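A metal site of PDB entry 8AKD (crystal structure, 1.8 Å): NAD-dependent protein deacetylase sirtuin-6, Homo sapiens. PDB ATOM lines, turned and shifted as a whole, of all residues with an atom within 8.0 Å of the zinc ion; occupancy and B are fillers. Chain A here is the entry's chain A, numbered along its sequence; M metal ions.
The side-chain sulfur of Cys 138 lies close to the side-chain hydroxyl of Thr 140.
The side-chain sulfur (SG) of Cys 135 sits close to the backbone NH (N) of Lys 137.
The backbone carbonyl oxygen (O) of Thr 140 is in hydrogen-bond range of the backbone NH (N) of Cys 135, 3.0 Å away.
The backbone NH (N) of Cys 160 is in hydrogen-bond range of the backbone carbonyl oxygen (O) of Gly 173, at 2.7 Å.
The side-chain hydroxyl of Tyr 142 lies close to the side-chain sulfur of Cys 160 (2.9 Å).
The backbone carbonyl oxygen (O) of Cys 160 lies within hydrogen-bond range of the backbone NH (N) of Arg 172 (3.3 Å).
N of Gly 173 sits close to SG of Cys 171, at 3.5 Å.
O of Cys 171 lies within hydrogen-bond range of NZ of Lys 137 (3.4 Å).
Within 4 Å of the zinc ion: Cys 135, Cys 138, Cys 160 and Cys 171.
The nearest printed residue that does not touch the zinc ion is Gly 173 (4.5 Å).
The zinc ion is bound by the side-chain sulfur of Cys 138 (2.2 Å), the side-chain sulfur of Cys 135 (2.3 Å), the side-chain sulfur of Cys 160 (2.3 Å) and the side-chain sulfur of Cys 171 (2.4 Å).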
ATOM      1  N   GLU A 134      17.963   0.163 -25.347  1.00  0.00           N
ATOM      2  CA  GLU A 134      17.926  -0.356 -26.742  1.00  0.00           C
ATOM      3  C   GLU A 134      16.634  -1.146 -26.905  1.00  0.00           C
ATOM      4  O   GLU A 134      16.267  -1.875 -25.972  1.00  0.00           O
ATOM      5  CB  GLU A 134      19.167  -1.217 -26.982  1.00  0.00           C
ATOM      6  CG  GLU A 134      19.253  -1.828 -28.367  1.00  0.00           C
ATOM      7  CD  GLU A 134      20.484  -2.701 -28.521  1.00  0.00           C
ATOM      8  OE1 GLU A 134      21.550  -2.156 -28.868  1.00  0.00           O
ATOM      9  OE2 GLU A 134      20.376  -3.920 -28.241  1.00  0.00           O
ATOM     10  N   CYS A 135      15.960  -0.986 -28.033  1.00  0.00           N
ATOM     11  CA  CYS A 135      14.710  -1.706 -28.362  1.00  0.00           C
ATOM     12  C   CYS A 135      15.077  -3.136 -28.776  1.00  0.00           C
ATOM     13  O   CYS A 135      15.919  -3.298 -29.669  1.00  0.00           O
ATOM     14  CB  CYS A 135      13.960  -0.993 -29.473  1.00  0.00           C
ATOM     15  SG  CYS A 135      12.503  -1.872 -30.101  1.00  0.00           S
ATOM     16  N   ALA A 136      14.487  -4.140 -28.136  1.00  0.00           N
ATOM     17  CA  ALA A 136      14.717  -5.558 -28.489  1.00  0.00           C
ATOM     18  C   ALA A 136      14.214  -5.815 -29.921  1.00  0.00           C
ATOM     19  O   ALA A 136      14.847  -6.609 -30.634  1.00  0.00           O
ATOM     20  CB  ALA A 136      14.044  -6.450 -27.500  1.00  0.00           C
ATOM     21  N   LYS A 137      13.114  -5.169 -30.314  1.00  0.00           N
ATOM     22  CA  LYS A 137      12.476  -5.367 -31.649  1.00  0.00           C
ATOM     23  C   LYS A 137      13.312  -4.728 -32.762  1.00  0.00           C
ATOM     24  O   LYS A 137      13.688  -5.468 -33.689  1.00  0.00           O
ATOM     25  CB  LYS A 137      11.068  -4.781 -31.699  1.00  0.00           C
ATOM     26  CG  LYS A 137       9.973  -5.616 -31.052  1.00  0.00           C
ATOM     27  CD  LYS A 137       8.595  -5.123 -31.418  1.00  0.00           C
ATOM     28  CE  LYS A 137       7.480  -5.938 -30.802  1.00  0.00           C
ATOM     29  NZ  LYS A 137       6.149  -5.376 -31.146  1.00  0.00           N
ATOM     30  N   CYS A 138      13.585  -3.413 -32.699  1.00  0.00           N
ATOM     31  CA  CYS A 138      14.182  -2.677 -33.845  1.00  0.00           C
ATOM     32  C   CYS A 138      15.642  -2.256 -33.574  1.00  0.00           C
ATOM     33  O   CYS A 138      16.230  -1.646 -34.476  1.00  0.00           O
ATOM     34  CB  CYS A 138      13.348  -1.477 -34.252  1.00  0.00           C
ATOM     35  SG  CYS A 138      13.361  -0.085 -33.088  1.00  0.00           S
ATOM     36  N   LYS A 139      16.190  -2.568 -32.395  1.00  0.00           N
ATOM     37  CA  LYS A 139      17.605  -2.307 -32.025  1.00  0.00           C
ATOM     38  C   LYS A 139      17.883  -0.801 -31.983  1.00  0.00           C
ATOM     39  O   LYS A 139      19.075  -0.428 -31.995  1.00  0.00           O
ATOM     40  CB  LYS A 139      18.547  -3.021 -33.012  1.00  0.00           C
ATOM     41  CG  LYS A 139      18.240  -4.500 -33.218  1.00  0.00           C
ATOM     42  CD  LYS A 139      18.217  -5.297 -31.930  1.00  0.00           C
ATOM     43  CE  LYS A 139      18.001  -6.782 -32.164  1.00  0.00           C
ATOM     44  NZ  LYS A 139      17.928  -7.520 -30.883  1.00  0.00           N
ATOM     45  N   THR A 140      16.852   0.046 -31.889  1.00  0.00           N
ATOM     46  CA  THR A 140      17.052   1.517 -31.868  1.00  0.00           C
ATOM     47  C   THR A 140      17.486   1.898 -30.459  1.00  0.00           C
ATOM     48  O   THR A 140      16.771   1.530 -29.518  1.00  0.00           O
ATOM     49  CB  THR A 140      15.818   2.296 -32.309  1.00  0.00           C
ATOM     50  OG1 THR A 140      15.683   2.149 -33.715  1.00  0.00           O
ATOM     51  CG2 THR A 140      15.917   3.772 -31.984  1.00  0.00           C
ATOM     52  N   GLN A 141      18.625   2.588 -30.335  1.00  0.00           N
ATOM     53  CA  GLN A 141      19.187   3.015 -29.030  1.00  0.00           C
ATOM     54  C   GLN A 141      18.712   4.422 -28.686  1.00  0.00           C
ATOM     55  O   GLN A 141      18.555   5.245 -29.617  1.00  0.00           O
ATOM     56  CB  GLN A 141      20.712   2.918 -29.040  1.00  0.00           C
ATOM     57  CG  GLN A 141      21.202   1.480 -29.096  1.00  0.00           C
ATOM     58  CD  GLN A 141      22.701   1.357 -29.103  1.00  0.00           C
ATOM     59  OE1 GLN A 141      23.414   2.240 -29.574  1.00  0.00           O
ATOM     60  NE2 GLN A 141      23.198   0.248 -28.573  1.00  0.00           N
ATOM     61  N   TYR A 142      18.472   4.660 -27.408  1.00  0.00           N
ATOM     62  CA  TYR A 142      18.068   5.961 -26.827  1.00  0.00           C
ATOM     63  C   TYR A 142      19.157   6.359 -25.835  1.00  0.00           C
ATOM     64  O   TYR A 142      19.493   5.519 -24.968  1.00  0.00           O
ATOM     65  CB  TYR A 142      16.717   5.856 -26.132  1.00  0.00           C
ATOM     66  CG  TYR A 142      15.567   5.438 -27.019  1.00  0.00           C
ATOM     67  CD1 TYR A 142      15.470   4.145 -27.501  1.00  0.00           C
ATOM     68  CD2 TYR A 142      14.564   6.339 -27.374  1.00  0.00           C
ATOM     69  CE1 TYR A 142      14.415   3.748 -28.301  1.00  0.00           C
ATOM     70  CE2 TYR A 142      13.498   5.961 -28.176  1.00  0.00           C
ATOM     71  CZ  TYR A 142      13.429   4.662 -28.643  1.00  0.00           C
ATOM     72  OH  TYR A 142      12.378   4.279 -29.429  1.00  0.00           O
ATOM     73  N   LEU A 159       8.941   1.812 -23.535  1.00  0.00           N
ATOM     74  CA  LEU A 159       8.642   1.183 -24.849  1.00  0.00           C
ATOM     75  C   LEU A 159       9.165   2.083 -25.959  1.00  0.00           C
ATOM     76  O   LEU A 159       9.263   3.311 -25.756  1.00  0.00           O
ATOM     77  CB  LEU A 159       7.130   0.944 -25.006  1.00  0.00           C
ATOM     78  CG  LEU A 159       6.503  -0.064 -24.038  1.00  0.00           C
ATOM     79  CD1 LEU A 159       5.018  -0.240 -24.350  1.00  0.00           C
ATOM     80  CD2 LEU A 159       7.223  -1.406 -24.083  1.00  0.00           C
ATOM     81  N   CYS A 160       9.460   1.473 -27.102  1.00  0.00           N
ATOM     82  CA  CYS A 160      10.024   2.150 -28.297  1.00  0.00           C
ATOM     83  C   CYS A 160       8.992   3.139 -28.865  1.00  0.00           C
ATOM     84  O   CYS A 160       7.797   2.827 -28.813  1.00  0.00           O
ATOM     85  CB  CYS A 160      10.387   1.126 -29.352  1.00  0.00           C
ATOM     86  SG  CYS A 160      11.560   1.772 -30.572  1.00  0.00           S
ATOM     87  N   THR A 161       9.459   4.272 -29.378  1.00  0.00           N
ATOM     88  CA  THR A 161       8.604   5.374 -29.882  1.00  0.00           C
ATOM     89  C   THR A 161       8.930   5.669 -31.358  1.00  0.00           C
ATOM     90  O   THR A 161       8.466   6.702 -31.861  1.00  0.00           O
ATOM     91  CB  THR A 161       8.741   6.609 -28.989  1.00  0.00           C
ATOM     92  OG1 THR A 161      10.111   7.007 -28.964  1.00  0.00           O
ATOM     93  CG2 THR A 161       8.262   6.365 -27.574  1.00  0.00           C
ATOM     94  N   VAL A 162       9.689   4.785 -32.020  1.00  0.00           N
ATOM     95  CA  VAL A 162      10.033   4.952 -33.471  1.00  0.00           C
ATOM     96  C   VAL A 162       8.748   4.910 -34.309  1.00  0.00           C
ATOM     97  O   VAL A 162       7.843   4.135 -33.964  1.00  0.00           O
ATOM     98  CB  VAL A 162      11.069   3.900 -33.921  1.00  0.00           C
ATOM     99  CG1 VAL A 162      11.169   3.787 -35.425  1.00  0.00           C
ATOM    100  CG2 VAL A 162      12.438   4.178 -33.312  1.00  0.00           C
ATOM    101  N   ALA A 163       8.695   5.722 -35.380  1.00  0.00           N
ATOM    102  CA  ALA A 163       7.514   5.921 -36.252  1.00  0.00           C
ATOM    103  C   ALA A 163       7.051   4.560 -36.818  1.00  0.00           C
ATOM    104  O   ALA A 163       7.888   3.916 -37.480  1.00  0.00           O
ATOM    105  CB  ALA A 163       7.827   6.898 -37.353  1.00  0.00           C
ATOM    106  N   CYS A 171       6.560   0.998 -33.060  1.00  0.00           N
ATOM    107  CA  CYS A 171       7.281  -0.259 -32.716  1.00  0.00           C
ATOM    108  C   CYS A 171       6.822  -0.743 -31.335  1.00  0.00           C
ATOM    109  O   CYS A 171       6.568  -1.963 -31.196  1.00  0.00           O
ATOM    110  CB  CYS A 171       8.790  -0.025 -32.711  1.00  0.00           C
ATOM    111  SG  CYS A 171       9.726  -1.474 -32.162  1.00  0.00           S
ATOM    112  N   ARG A 172       6.745   0.171 -30.374  1.00  0.00           N
ATOM    113  CA  ARG A 172       6.318  -0.105 -28.967  1.00  0.00           C
ATOM    114  C   ARG A 172       7.102  -1.310 -28.430  1.00  0.00           C
ATOM    115  O   ARG A 172       6.630  -1.941 -27.460  1.00  0.00           O
ATOM    116  CB  ARG A 172       4.798  -0.291 -28.917  1.00  0.00           C
ATOM    117  CG  ARG A 172       4.018   0.872 -29.513  1.00  0.00           C
ATOM    118  CD  ARG A 172       2.957   1.433 -28.575  1.00  0.00           C
ATOM    119  NE  ARG A 172       1.780   0.581 -28.484  1.00  0.00           N
ATOM    120  CZ  ARG A 172       1.394  -0.106 -27.403  1.00  0.00           C
ATOM    121  NH1 ARG A 172       2.090  -0.057 -26.276  1.00  0.00           N
ATOM    122  NH2 ARG A 172       0.301  -0.850 -27.467  1.00  0.00           N
ATOM    123  N   GLY A 173       8.272  -1.578 -28.997  1.00  0.00           N
ATOM    124  CA  GLY A 173       9.183  -2.653 -28.561  1.00  0.00           C
ATOM    125  C   GLY A 173       9.724  -2.367 -27.167  1.00  0.00           C
ATOM    126  O   GLY A 173       9.800  -1.172 -26.781  1.00  0.00           O
ATOM    127  N   GLU A 174      10.061  -3.436 -26.442  1.00  0.00           N
ATOM    128  CA  GLU A 174      10.537  -3.400 -25.040  1.00  0.00           C
ATOM    129  C   GLU A 174      11.937  -2.788 -25.021  1.00  0.00           C
ATOM    130  O   GLU A 174      12.839  -3.398 -25.645  1.00  0.00           O
ATOM    131  CB  GLU A 174      10.520  -4.822 -24.458  1.00  0.00           C
ATOM    132  CG  GLU A 174      10.766  -4.886 -22.962  1.00  0.00           C
ATOM    133  CD  GLU A 174      10.622  -6.288 -22.389  1.00  0.00           C
ATOM    134  OE1 GLU A 174       9.651  -6.515 -21.636  1.00  0.00           O
ATOM    135  OE2 GLU A 174      11.498  -7.132 -22.669  1.00  0.00           O
ATOM    136  N   LEU A 175      12.110  -1.630 -24.388  1.00  0.00           N
ATOM    137  CA  LEU A 175      13.440  -1.009 -24.149  1.00  0.00           C
ATOM    138  C   LEU A 175      14.153  -1.782 -23.041  1.00  0.00           C
ATOM    139  O   LEU A 175      13.523  -2.058 -21.994  1.00  0.00           O
ATOM    140  CB  LEU A 175      13.291   0.461 -23.779  1.00  0.00           C
ATOM    141  CG  LEU A 175      12.703   1.352 -24.874  1.00  0.00           C
ATOM    142  CD1 LEU A 175      12.979   2.824 -24.568  1.00  0.00           C
ATOM    143  CD2 LEU A 175      13.248   0.990 -26.250  1.00  0.00           C
HETATM  144 ZN    ZN M   1      11.736  -0.323 -31.566  1.00  0.00          ZN
